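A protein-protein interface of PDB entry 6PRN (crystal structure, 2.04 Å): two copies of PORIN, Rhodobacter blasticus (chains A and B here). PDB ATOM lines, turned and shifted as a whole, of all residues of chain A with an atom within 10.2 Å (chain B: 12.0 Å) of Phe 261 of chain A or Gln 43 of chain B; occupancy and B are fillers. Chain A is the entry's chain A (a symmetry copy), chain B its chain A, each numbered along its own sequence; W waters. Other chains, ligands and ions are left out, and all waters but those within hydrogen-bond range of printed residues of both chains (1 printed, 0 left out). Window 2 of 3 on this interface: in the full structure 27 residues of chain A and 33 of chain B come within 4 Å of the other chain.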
ATOM      1  N   GLY A 233     -10.443 -43.280  32.227  1.00  0.00           N
ATOM      2  CA  GLY A 233      -9.147 -42.581  32.142  1.00  0.00           C
ATOM      3  C   GLY A 233      -9.418 -41.062  31.993  1.00  0.00           C
ATOM      4  O   GLY A 233     -10.050 -40.489  32.894  1.00  0.00           O
ATOM      5  N   ALA A 234      -8.959 -40.482  30.906  1.00  0.00           N
ATOM      6  CA  ALA A 234      -9.130 -39.044  30.688  1.00  0.00           C
ATOM      7  C   ALA A 234     -10.452 -38.690  30.009  1.00  0.00           C
ATOM      8  O   ALA A 234     -10.762 -37.508  29.808  1.00  0.00           O
ATOM      9  CB  ALA A 234      -7.979 -38.487  29.843  1.00  0.00           C
ATOM     10  N   THR A 235     -11.212 -39.699  29.551  1.00  0.00           N
ATOM     11  CA  THR A 235     -12.471 -39.356  28.897  1.00  0.00           C
ATOM     12  C   THR A 235     -13.676 -39.737  29.713  1.00  0.00           C
ATOM     13  O   THR A 235     -13.763 -40.817  30.328  1.00  0.00           O
ATOM     14  CB  THR A 235     -12.560 -39.694  27.430  1.00  0.00           C
ATOM     15  OG1 THR A 235     -13.827 -40.296  27.095  1.00  0.00           O
ATOM     16  CG2 THR A 235     -11.399 -40.378  26.840  1.00  0.00           C
ATOM     17  N   THR A 236     -14.616 -38.787  29.784  1.00  0.00           N
ATOM     18  CA  THR A 236     -15.852 -38.953  30.512  1.00  0.00           C
ATOM     19  C   THR A 236     -17.024 -39.000  29.503  1.00  0.00           C
ATOM     20  O   THR A 236     -17.094 -38.175  28.576  1.00  0.00           O
ATOM     21  CB  THR A 236     -16.091 -37.839  31.512  1.00  0.00           C
ATOM     22  OG1 THR A 236     -15.015 -37.744  32.439  1.00  0.00           O
ATOM     23  CG2 THR A 236     -17.381 -38.015  32.311  1.00  0.00           C
ATOM     24  N   ALA A 257     -19.450 -36.161  25.538  1.00  0.00           N
ATOM     25  CA  ALA A 257     -18.182 -36.678  26.122  1.00  0.00           C
ATOM     26  C   ALA A 257     -17.224 -35.512  26.401  1.00  0.00           C
ATOM     27  O   ALA A 257     -17.255 -34.483  25.697  1.00  0.00           O
ATOM     28  CB  ALA A 257     -17.557 -37.635  25.144  1.00  0.00           C
ATOM     29  N   ASP A 258     -16.452 -35.670  27.457  1.00  0.00           N
ATOM     30  CA  ASP A 258     -15.401 -34.739  27.807  1.00  0.00           C
ATOM     31  C   ASP A 258     -14.035 -35.477  27.732  1.00  0.00           C
ATOM     32  O   ASP A 258     -13.923 -36.641  28.182  1.00  0.00           O
ATOM     33  CB  ASP A 258     -15.508 -34.198  29.212  1.00  0.00           C
ATOM     34  CG  ASP A 258     -16.840 -33.580  29.599  1.00  0.00           C
ATOM     35  OD1 ASP A 258     -17.449 -32.909  28.762  1.00  0.00           O
ATOM     36  OD2 ASP A 258     -17.263 -33.759  30.758  1.00  0.00           O
ATOM     37  N   TYR A 259     -13.053 -34.755  27.251  1.00  0.00           N
ATOM     38  CA  TYR A 259     -11.685 -35.277  27.234  1.00  0.00           C
ATOM     39  C   TYR A 259     -10.795 -34.288  28.002  1.00  0.00           C
ATOM     40  O   TYR A 259     -10.731 -33.094  27.610  1.00  0.00           O
ATOM     41  CB  TYR A 259     -11.231 -35.494  25.796  1.00  0.00           C
ATOM     42  CG  TYR A 259      -9.805 -36.040  25.740  1.00  0.00           C
ATOM     43  CD1 TYR A 259      -9.595 -37.365  26.115  1.00  0.00           C
ATOM     44  CD2 TYR A 259      -8.719 -35.290  25.341  1.00  0.00           C
ATOM     45  CE1 TYR A 259      -8.330 -37.919  26.094  1.00  0.00           C
ATOM     46  CE2 TYR A 259      -7.441 -35.839  25.303  1.00  0.00           C
ATOM     47  CZ  TYR A 259      -7.263 -37.147  25.681  1.00  0.00           C
ATOM     48  OH  TYR A 259      -6.011 -37.740  25.675  1.00  0.00           O
ATOM     49  N   GLN A 260     -10.159 -34.765  29.051  1.00  0.00           N
ATOM     50  CA  GLN A 260      -9.254 -33.894  29.850  1.00  0.00           C
ATOM     51  C   GLN A 260      -7.903 -33.881  29.151  1.00  0.00           C
ATOM     52  O   GLN A 260      -7.034 -34.767  29.344  1.00  0.00           O
ATOM     53  CB  GLN A 260      -9.208 -34.350  31.282  1.00  0.00           C
ATOM     54  CG  GLN A 260      -8.638 -33.413  32.335  1.00  0.00           C
ATOM     55  CD  GLN A 260      -9.560 -32.225  32.607  1.00  0.00           C
ATOM     56  OE1 GLN A 260     -10.776 -32.411  32.804  1.00  0.00           O
ATOM     57  NE2 GLN A 260      -9.027 -31.001  32.595  1.00  0.00           N
ATOM     58  N   PHE A 261      -7.690 -32.920  28.285  1.00  0.00           N
ATOM     59  CA  PHE A 261      -6.466 -32.794  27.525  1.00  0.00           C
ATOM     60  C   PHE A 261      -5.258 -32.545  28.442  1.00  0.00           C
ATOM     61  O   PHE A 261      -4.178 -33.067  28.166  1.00  0.00           O
ATOM     62  CB  PHE A 261      -6.602 -31.687  26.480  1.00  0.00           C
ATOM     63  CG  PHE A 261      -5.406 -31.488  25.600  1.00  0.00           C
ATOM     64  CD1 PHE A 261      -5.105 -32.426  24.618  1.00  0.00           C
ATOM     65  CD2 PHE A 261      -4.571 -30.404  25.733  1.00  0.00           C
ATOM     66  CE1 PHE A 261      -3.991 -32.280  23.797  1.00  0.00           C
ATOM     67  CE2 PHE A 261      -3.471 -30.225  24.928  1.00  0.00           C
ATOM     68  CZ  PHE A 261      -3.183 -31.159  23.947  1.00  0.00           C
ATOM     69  N   ALA A 262      -5.422 -31.710  29.445  1.00  0.00           N
ATOM     70  CA  ALA A 262      -4.358 -31.368  30.371  1.00  0.00           C
ATOM     71  C   ALA A 262      -5.016 -30.708  31.558  1.00  0.00           C
ATOM     72  O   ALA A 262      -6.262 -30.501  31.481  1.00  0.00           O
ATOM     73  CB  ALA A 262      -3.321 -30.425  29.752  1.00  0.00           C
ATOM     74  N   GLU A 263      -4.280 -30.416  32.598  1.00  0.00           N
ATOM     75  CA  GLU A 263      -4.849 -29.707  33.729  1.00  0.00           C
ATOM     76  C   GLU A 263      -5.398 -28.354  33.161  1.00  0.00           C
ATOM     77  O   GLU A 263      -4.641 -27.680  32.420  1.00  0.00           O
ATOM     78  CB  GLU A 263      -3.782 -29.376  34.768  1.00  0.00           C
ATOM     79  CG  GLU A 263      -4.330 -28.615  35.969  1.00  0.00           C
ATOM     80  CD  GLU A 263      -3.270 -28.354  37.038  1.00  0.00           C
ATOM     81  OE1 GLU A 263      -2.192 -29.018  37.040  1.00  0.00           O
ATOM     82  OE2 GLU A 263      -3.531 -27.464  37.902  1.00  0.00           O
ATOM     83  N   GLY A 264      -6.607 -28.014  33.477  1.00  0.00           N
ATOM     84  CA  GLY A 264      -7.176 -26.763  32.989  1.00  0.00           C
ATOM     85  C   GLY A 264      -7.610 -26.744  31.532  1.00  0.00           C
ATOM     86  O   GLY A 264      -7.957 -25.631  31.067  1.00  0.00           O
ATOM     87  N   VAL A 265      -7.549 -27.833  30.753  1.00  0.00           N
ATOM     88  CA  VAL A 265      -7.939 -27.789  29.356  1.00  0.00           C
ATOM     89  C   VAL A 265      -8.903 -28.964  29.094  1.00  0.00           C
ATOM     90  O   VAL A 265      -8.478 -30.135  29.284  1.00  0.00           O
ATOM     91  CB  VAL A 265      -6.812 -27.818  28.334  1.00  0.00           C
ATOM     92  CG1 VAL A 265      -7.360 -27.753  26.889  1.00  0.00           C
ATOM     93  CG2 VAL A 265      -5.799 -26.686  28.526  1.00  0.00           C
ATOM     94  N   LYS A 266     -10.140 -28.642  28.726  1.00  0.00           N
ATOM     95  CA  LYS A 266     -11.123 -29.740  28.537  1.00  0.00           C
ATOM     96  C   LYS A 266     -11.742 -29.638  27.178  1.00  0.00           C
ATOM     97  O   LYS A 266     -12.185 -28.532  26.738  1.00  0.00           O
ATOM     98  CB  LYS A 266     -12.099 -29.697  29.696  1.00  0.00           C
ATOM     99  CG  LYS A 266     -13.336 -30.522  29.654  1.00  0.00           C
ATOM    100  CD  LYS A 266     -13.936 -30.683  31.054  1.00  0.00           C
ATOM    101  CE  LYS A 266     -15.169 -29.818  31.207  1.00  0.00           C
ATOM    102  NZ  LYS A 266     -15.947 -30.225  32.446  1.00  0.00           N
ATOM    103  N   VAL A 267     -11.714 -30.724  26.403  1.00  0.00           N
ATOM    104  CA  VAL A 267     -12.360 -30.751  25.085  1.00  0.00           C
ATOM    105  C   VAL A 267     -13.710 -31.441  25.241  1.00  0.00           C
ATOM    106  O   VAL A 267     -13.768 -32.468  25.972  1.00  0.00           O
ATOM    107  CB  VAL A 267     -11.510 -31.483  24.058  1.00  0.00           C
ATOM    108  CG1 VAL A 267     -12.140 -31.406  22.646  1.00  0.00           C
ATOM    109  CG2 VAL A 267     -10.136 -30.821  24.036  1.00  0.00           C
ATOM    110  N   SER A 268     -14.819 -30.816  24.803  1.00  0.00           N
ATOM    111  CA  SER A 268     -16.100 -31.456  25.078  1.00  0.00           C
ATOM    112  C   SER A 268     -17.043 -31.268  23.899  1.00  0.00           C
ATOM    113  O   SER A 268     -16.921 -30.307  23.132  1.00  0.00           O
ATOM    114  CB  SER A 268     -16.928 -30.864  26.223  1.00  0.00           C
ATOM    115  OG  SER A 268     -16.127 -30.716  27.384  1.00  0.00           O
ATOM    116  N   GLY A 284     -16.142 -28.266  21.322  1.00  0.00           N
ATOM    117  CA  GLY A 284     -15.210 -27.164  21.558  1.00  0.00           C
ATOM    118  C   GLY A 284     -14.265 -27.444  22.700  1.00  0.00           C
ATOM    119  O   GLY A 284     -14.214 -28.543  23.280  1.00  0.00           O
ATOM    120  N   VAL A 285     -13.574 -26.377  23.115  1.00  0.00           N
ATOM    121  CA  VAL A 285     -12.603 -26.481  24.197  1.00  0.00           C
ATOM    122  C   VAL A 285     -12.796 -25.375  25.210  1.00  0.00           C
ATOM    123  O   VAL A 285     -13.210 -24.263  24.823  1.00  0.00           O
ATOM    124  CB  VAL A 285     -11.174 -26.428  23.575  1.00  0.00           C
ATOM    125  CG1 VAL A 285     -10.946 -25.110  22.844  1.00  0.00           C
ATOM    126  CG2 VAL A 285     -10.103 -26.524  24.679  1.00  0.00           C
ATOM    127  N   ARG A 286     -12.604 -25.672  26.471  1.00  0.00           N
ATOM    128  CA  ARG A 286     -12.589 -24.665  27.526  1.00  0.00           C
ATOM    129  C   ARG A 286     -11.178 -24.702  28.142  1.00  0.00           C
ATOM    130  O   ARG A 286     -10.677 -25.813  28.449  1.00  0.00           O
ATOM    131  CB  ARG A 286     -13.639 -24.979  28.618  1.00  0.00           C
ATOM    132  CG  ARG A 286     -13.434 -23.997  29.830  1.00  0.00           C
ATOM    133  CD  ARG A 286     -14.456 -24.261  30.931  1.00  0.00           C
ATOM    134  NE  ARG A 286     -13.984 -23.669  32.222  1.00  0.00           N
ATOM    135  CZ  ARG A 286     -14.747 -23.107  33.125  1.00  0.00           C
ATOM    136  NH1 ARG A 286     -16.060 -23.017  32.889  1.00  0.00           N
ATOM    137  NH2 ARG A 286     -14.291 -22.579  34.271  1.00  0.00           N
ATOM    138  N   PHE A 287     -10.539 -23.574  28.381  1.00  0.00           N
ATOM    139  CA  PHE A 287      -9.253 -23.561  29.050  1.00  0.00           C
ATOM    140  C   PHE A 287      -9.322 -22.531  30.184  1.00  0.00           C
ATOM    141  O   PHE A 287      -9.884 -21.438  30.001  1.00  0.00           O
ATOM    142  CB  PHE A 287      -8.133 -23.310  28.059  1.00  0.00           C
ATOM    143  CG  PHE A 287      -8.337 -22.093  27.154  1.00  0.00           C
ATOM    144  CD1 PHE A 287      -9.045 -22.181  25.984  1.00  0.00           C
ATOM    145  CD2 PHE A 287      -7.745 -20.893  27.515  1.00  0.00           C
ATOM    146  CE1 PHE A 287      -9.177 -21.067  25.147  1.00  0.00           C
ATOM    147  CE2 PHE A 287      -7.888 -19.772  26.704  1.00  0.00           C
ATOM    148  CZ  PHE A 287      -8.647 -19.868  25.544  1.00  0.00           C
ATOM    149  N   THR B  38      -3.454 -17.093  29.641  1.00  0.00           N
ATOM    150  CA  THR B  38      -2.812 -18.175  28.883  1.00  0.00           C
ATOM    151  C   THR B  38      -2.804 -19.454  29.725  1.00  0.00           C
ATOM    152  O   THR B  38      -2.682 -19.419  30.932  1.00  0.00           O
ATOM    153  CB  THR B  38      -1.333 -17.941  28.468  1.00  0.00           C
ATOM    154  OG1 THR B  38      -0.603 -17.536  29.603  1.00  0.00           O
ATOM    155  CG2 THR B  38      -1.211 -16.845  27.418  1.00  0.00           C
ATOM    156  N   THR B  39      -2.962 -20.579  29.048  1.00  0.00           N
ATOM    157  CA  THR B  39      -2.944 -21.887  29.693  1.00  0.00           C
ATOM    158  C   THR B  39      -1.867 -22.712  28.935  1.00  0.00           C
ATOM    159  O   THR B  39      -2.072 -23.002  27.752  1.00  0.00           O
ATOM    160  CB  THR B  39      -4.292 -22.612  29.568  1.00  0.00           C
ATOM    161  OG1 THR B  39      -5.323 -21.764  30.117  1.00  0.00           O
ATOM    162  CG2 THR B  39      -4.230 -23.923  30.376  1.00  0.00           C
ATOM    163  N   GLU B  40      -0.797 -23.014  29.618  1.00  0.00           N
ATOM    164  CA  GLU B  40       0.285 -23.805  28.969  1.00  0.00           C
ATOM    165  C   GLU B  40       0.061 -25.272  29.323  1.00  0.00           C
ATOM    166  O   GLU B  40      -0.634 -25.582  30.334  1.00  0.00           O
ATOM    167  CB  GLU B  40       1.635 -23.326  29.512  1.00  0.00           C
ATOM    168  CG  GLU B  40       1.907 -21.871  29.036  1.00  0.00           C
ATOM    169  CD  GLU B  40       3.166 -21.309  29.703  1.00  0.00           C
ATOM    170  OE1 GLU B  40       3.853 -22.023  30.472  1.00  0.00           O
ATOM    171  OE2 GLU B  40       3.485 -20.105  29.422  1.00  0.00           O
ATOM    172  N   THR B  41       0.444 -26.173  28.418  1.00  0.00           N
ATOM    173  CA  THR B  41       0.195 -27.590  28.703  1.00  0.00           C
ATOM    174  C   THR B  41       1.557 -28.336  28.593  1.00  0.00           C
ATOM    175  O   THR B  41       2.414 -27.902  27.827  1.00  0.00           O
ATOM    176  CB  THR B  41      -0.812 -28.293  27.806  1.00  0.00           C
ATOM    177  OG1 THR B  41      -0.369 -28.284  26.450  1.00  0.00           O
ATOM    178  CG2 THR B  41      -2.205 -27.592  27.826  1.00  0.00           C
ATOM    179  N   ASP B  42       1.640 -29.504  29.204  1.00  0.00           N
ATOM    180  CA  ASP B  42       2.911 -30.255  29.084  1.00  0.00           C
ATOM    181  C   ASP B  42       3.039 -30.890  27.707  1.00  0.00           C
ATOM    182  O   ASP B  42       4.123 -31.321  27.364  1.00  0.00           O
ATOM    183  CB  ASP B  42       3.163 -31.194  30.212  1.00  0.00           C
ATOM    184  CG  ASP B  42       2.120 -32.233  30.454  1.00  0.00           C
ATOM    185  OD1 ASP B  42       1.257 -32.479  29.613  1.00  0.00           O
ATOM    186  OD2 ASP B  42       2.173 -32.873  31.516  1.00  0.00           O
ATOM    187  N   GLN B  43       1.982 -30.887  26.897  1.00  0.00           N
ATOM    188  CA  GLN B  43       2.017 -31.408  25.562  1.00  0.00           C
ATOM    189  C   GLN B  43       2.632 -30.357  24.623  1.00  0.00           C
ATOM    190  O   GLN B  43       2.838 -30.621  23.433  1.00  0.00           O
ATOM    191  CB  GLN B  43       0.620 -31.804  25.071  1.00  0.00           C
ATOM    192  CG  GLN B  43      -0.239 -32.498  26.163  1.00  0.00           C
ATOM    193  CD  GLN B  43       0.314 -33.891  26.411  1.00  0.00           C
ATOM    194  OE1 GLN B  43       0.660 -34.598  25.451  1.00  0.00           O
ATOM    195  NE2 GLN B  43       0.447 -34.368  27.663  1.00  0.00           N
ATOM    196  N   GLY B  44       2.834 -29.135  25.100  1.00  0.00           N
ATOM    197  CA  GLY B  44       3.413 -28.090  24.251  1.00  0.00           C
ATOM    198  C   GLY B  44       2.353 -27.311  23.470  1.00  0.00           C
ATOM    199  O   GLY B  44       2.734 -26.536  22.572  1.00  0.00           O
ATOM    200  N   VAL B  45       1.077 -27.486  23.777  1.00  0.00           N
ATOM    201  CA  VAL B  45       0.024 -26.700  23.137  1.00  0.00           C
ATOM    202  C   VAL B  45      -0.330 -25.540  24.083  1.00  0.00           C
ATOM    203  O   VAL B  45      -0.650 -25.837  25.244  1.00  0.00           O
ATOM    204  CB  VAL B  45      -1.250 -27.503  22.882  1.00  0.00           C
ATOM    205  CG1 VAL B  45      -2.291 -26.654  22.148  1.00  0.00           C
ATOM    206  CG2 VAL B  45      -0.908 -28.737  22.007  1.00  0.00           C
ATOM    207  N   THR B  46      -0.243 -24.316  23.618  1.00  0.00           N
ATOM    208  CA  THR B  46      -0.611 -23.194  24.532  1.00  0.00           C
ATOM    209  C   THR B  46      -1.987 -22.673  24.111  1.00  0.00           C
ATOM    210  O   THR B  46      -2.243 -22.587  22.894  1.00  0.00           O
ATOM    211  CB  THR B  46       0.441 -22.091  24.391  1.00  0.00           C
ATOM    212  OG1 THR B  46       1.660 -22.592  24.943  1.00  0.00           O
ATOM    213  CG2 THR B  46       0.079 -20.851  25.242  1.00  0.00           C
ATOM    214  N   PHE B  47      -2.846 -22.378  25.050  1.00  0.00           N
ATOM    215  CA  PHE B  47      -4.159 -21.788  24.727  1.00  0.00           C
ATOM    216  C   PHE B  47      -4.127 -20.357  25.302  1.00  0.00           C
ATOM    217  O   PHE B  47      -3.516 -20.144  26.371  1.00  0.00           O
ATOM    218  CB  PHE B  47      -5.337 -22.553  25.314  1.00  0.00           C
ATOM    219  CG  PHE B  47      -5.464 -23.961  24.755  1.00  0.00           C
ATOM    220  CD1 PHE B  47      -4.686 -24.985  25.252  1.00  0.00           C
ATOM    221  CD2 PHE B  47      -6.386 -24.213  23.747  1.00  0.00           C
ATOM    222  CE1 PHE B  47      -4.804 -26.290  24.744  1.00  0.00           C
ATOM    223  CE2 PHE B  47      -6.511 -25.509  23.247  1.00  0.00           C
ATOM    224  CZ  PHE B  47      -5.728 -26.529  23.743  1.00  0.00           C
ATOM    225  N   GLY B  48      -4.702 -19.413  24.576  1.00  0.00           N
ATOM    226  CA  GLY B  48      -4.686 -18.047  25.074  1.00  0.00           C
ATOM    227  C   GLY B  48      -5.951 -17.292  24.665  1.00  0.00           C
ATOM    228  O   GLY B  48      -6.631 -17.651  23.700  1.00  0.00           O
ATOM    229  N   TRP B  72      -6.646 -18.037  20.916  1.00  0.00           N
ATOM    230  CA  TRP B  72      -5.683 -18.717  20.053  1.00  0.00           C
ATOM    231  C   TRP B  72      -5.187 -20.009  20.705  1.00  0.00           C
ATOM    232  O   TRP B  72      -5.287 -20.213  21.916  1.00  0.00           O
ATOM    233  CB  TRP B  72      -4.486 -17.882  19.640  1.00  0.00           C
ATOM    234  CG  TRP B  72      -3.584 -17.555  20.777  1.00  0.00           C
ATOM    235  CD1 TRP B  72      -2.494 -18.293  21.226  1.00  0.00           C
ATOM    236  CD2 TRP B  72      -3.670 -16.410  21.624  1.00  0.00           C
ATOM    237  NE1 TRP B  72      -1.933 -17.656  22.302  1.00  0.00           N
ATOM    238  CE2 TRP B  72      -2.633 -16.505  22.560  1.00  0.00           C
ATOM    239  CE3 TRP B  72      -4.554 -15.315  21.669  1.00  0.00           C
ATOM    240  CZ2 TRP B  72      -2.427 -15.536  23.554  1.00  0.00           C
ATOM    241  CZ3 TRP B  72      -4.356 -14.359  22.648  1.00  0.00           C
ATOM    242  CH2 TRP B  72      -3.300 -14.484  23.568  1.00  0.00           C
ATOM    243  N   THR B  73      -4.626 -20.848  19.817  1.00  0.00           N
ATOM    244  CA  THR B  73      -4.019 -22.104  20.181  1.00  0.00           C
ATOM    245  C   THR B  73      -2.700 -22.168  19.362  1.00  0.00           C
ATOM    246  O   THR B  73      -2.746 -21.882  18.153  1.00  0.00           O
ATOM    247  CB  THR B  73      -4.833 -23.333  19.769  1.00  0.00           C
ATOM    248  OG1 THR B  73      -6.203 -23.164  20.170  1.00  0.00           O
ATOM    249  CG2 THR B  73      -4.289 -24.572  20.468  1.00  0.00           C
ATOM    250  N   SER B  74      -1.609 -22.406  20.054  1.00  0.00           N
ATOM    251  CA  SER B  74      -0.292 -22.432  19.470  1.00  0.00           C
ATOM    252  C   SER B  74       0.416 -23.783  19.699  1.00  0.00           C
ATOM    253  O   SER B  74       0.396 -24.297  20.835  1.00  0.00           O
ATOM    254  CB  SER B  74       0.596 -21.343  20.091  1.00  0.00           C
ATOM    255  OG  SER B  74       0.121 -20.067  19.686  1.00  0.00           O
ATOM    256  N   TYR B  75       1.061 -24.262  18.624  1.00  0.00           N
ATOM    257  CA  TYR B  75       1.793 -25.530  18.710  1.00  0.00           C
ATOM    258  C   TYR B  75       2.861 -25.572  17.616  1.00  0.00           C
ATOM    259  O   TYR B  75       2.559 -25.379  16.436  1.00  0.00           O
ATOM    260  CB  TYR B  75       0.841 -26.706  18.501  1.00  0.00           C
ATOM    261  CG  TYR B  75       1.488 -28.074  18.617  1.00  0.00           C
ATOM    262  CD1 TYR B  75       2.148 -28.456  19.779  1.00  0.00           C
ATOM    263  CD2 TYR B  75       1.425 -28.980  17.568  1.00  0.00           C
ATOM    264  CE1 TYR B  75       2.730 -29.696  19.894  1.00  0.00           C
ATOM    265  CE2 TYR B  75       2.009 -30.240  17.666  1.00  0.00           C
ATOM    266  CZ  TYR B  75       2.658 -30.583  18.836  1.00  0.00           C
ATOM    267  OH  TYR B  75       3.246 -31.823  18.953  1.00  0.00           O
ATOM    268  N   ASN B  76       4.099 -25.753  18.036  1.00  0.00           N
ATOM    269  CA  ASN B  76       5.211 -25.921  17.092  1.00  0.00           C
ATOM    270  C   ASN B  76       5.348 -24.850  16.044  1.00  0.00           C
ATOM    271  O   ASN B  76       5.472 -25.199  14.842  1.00  0.00           O
ATOM    272  CB  ASN B  76       4.898 -27.255  16.333  1.00  0.00           C
ATOM    273  CG  ASN B  76       5.928 -28.312  16.699  1.00  0.00           C
ATOM    274  OD1 ASN B  76       5.853 -28.879  17.789  1.00  0.00           O
ATOM    275  ND2 ASN B  76       6.903 -28.586  15.859  1.00  0.00           N
ATOM    276  N   GLY B  77       5.284 -23.568  16.398  1.00  0.00           N
ATOM    277  CA  GLY B  77       5.440 -22.524  15.381  1.00  0.00           C
ATOM    278  C   GLY B  77       4.129 -22.136  14.706  1.00  0.00           C
ATOM    279  O   GLY B  77       4.062 -21.169  13.942  1.00  0.00           O
ATOM    280  N   VAL B  78       3.081 -22.926  14.867  1.00  0.00           N
ATOM    281  CA  VAL B  78       1.808 -22.667  14.233  1.00  0.00           C
ATOM    282  C   VAL B  78       0.824 -22.055  15.264  1.00  0.00           C
ATOM    283  O   VAL B  78       0.687 -22.600  16.356  1.00  0.00           O
ATOM    284  CB  VAL B  78       1.181 -23.954  13.687  1.00  0.00           C
ATOM    285  CG1 VAL B  78      -0.062 -23.641  12.882  1.00  0.00           C
ATOM    286  CG2 VAL B  78       2.185 -24.716  12.800  1.00  0.00           C
HETATM  287  O   HOH W   1      -2.115 -27.314  31.788  1.00  0.00           O
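The side-chain amide nitrogen (NE2) of Gln 260 of chain A lies within hydrogen-bond range of the backbone carbonyl oxygen (O) of Ala 262 of chain A (3.0 Å). The backbone NH of Thr 39 of chain B is in hydrogen-bond range of the backbone carbonyl oxygen of Phe 47 of chain B (2.8 Å). N of Trp 72 of chain B sits at hydrogen-bond distance from O of Gly 48 of chain B (2.8 Å). The side-chain carboxylate of Asp 42 of chain B lies within hydrogen-bond range of the side-chain amide nitrogen of Gln 43 of chain B. NE2 of Gln 260 of chain A sits at hydrogen-bond distance from O of Val 265 of chain A (3.5 Å). OG1 of Thr 41 of chain B lies within hydrogen-bond range of O of Val 45 of chain B, at 2.7 Å.
Thr 41 of chain B touches Phe 261 of chain A. Gln 43 of chain B touches Phe 261 of chain A. CZ of Phe 261 of chain A touches CG2 of Val 45 of chain B (3.8 Å). CB of Ala 262 of chain A touches CG2 of Thr 41 of chain B (3.6 Å). CG2 of Thr 39 of chain B touches CG2 of Val 265 of chain A (3.7 Å). CG2 of Val 265 of chain A touches CG2 of Thr 41 of chain B, at 3.8 Å. Phe 47 of chain B touches Val 265 of chain A (CE1 to CG1, 3.6 Å). CG2 of Val 285 of chain A touches CE2 of Phe 47 of chain B, at 3.998 Å. Phe 287 of chain A touches Thr 39 of chain B. Phe 287 of chain A touches Phe 47 of chain B.
Phe 261 of chain A touches three residues of chain B. Gln 43 of chain B touches one residue of chain A. No residue of chain B comes within 4 Å of Gln 260 of chain A. No residue of chain B comes within 4 Å of Gly 264 of chain A. Printed residues of chain B within 4 Å of Val 265 of chain A: Thr 39, Thr 41 and Phe 47. No residue of chain B comes within 4 Å of Val 267 of chain A. Of chain A, only Phe 261 (3.96 Å), Ala 262 (3.6 Å) and Val 265 (3.8 Å) come within 4 Å of Thr 41 of chain B. Val 45 of chain B touches just one residue of chain A: Phe 261 (3.8 Å). Of the printed residues of chain A, Thr 39 of chain B touches Val 265 and Phe 287. Printed residues of chain B within 4 Å of Phe 287 of chain A: Thr 39 (3.7 Å), Phe 47 (3.5 Å) and Gly 48 (3.5 Å). Printed residues of chain A within 4 Å of Phe 47 of chain B: Val 265, Val 285 and Phe 287. Of the printed residues of chain B, Val 285 of chain A touches Phe 47 (3.998 Å). Printed residues of chain A within 4 Å of Gly 48 of chain B: Phe 287 (3.5 Å). Ser 268 of chain A touches none of the printed residues of chain B. Asn 76 of chain B touches none of the printed residues of chain A. The nearest printed residue of chain A that does not touch Phe 47 of chain B is Phe 261 of chain A (4.2 Å).
Of the 18 printed residues of chain B, 6 touch a printed residue of chain A. Among the printed residues, no Asp or Glu carboxylate lies within 4 Å of a Lys or Arg side-chain nitrogen of the other chain.
No position is printed for both chains. Of the 11 pairs that touch across the chains among the printed residues, none has its exchanged pair printed and touching as well.
Water W1 bridges O of Glu 263 of chain A and O of Glu 40 of chain B.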
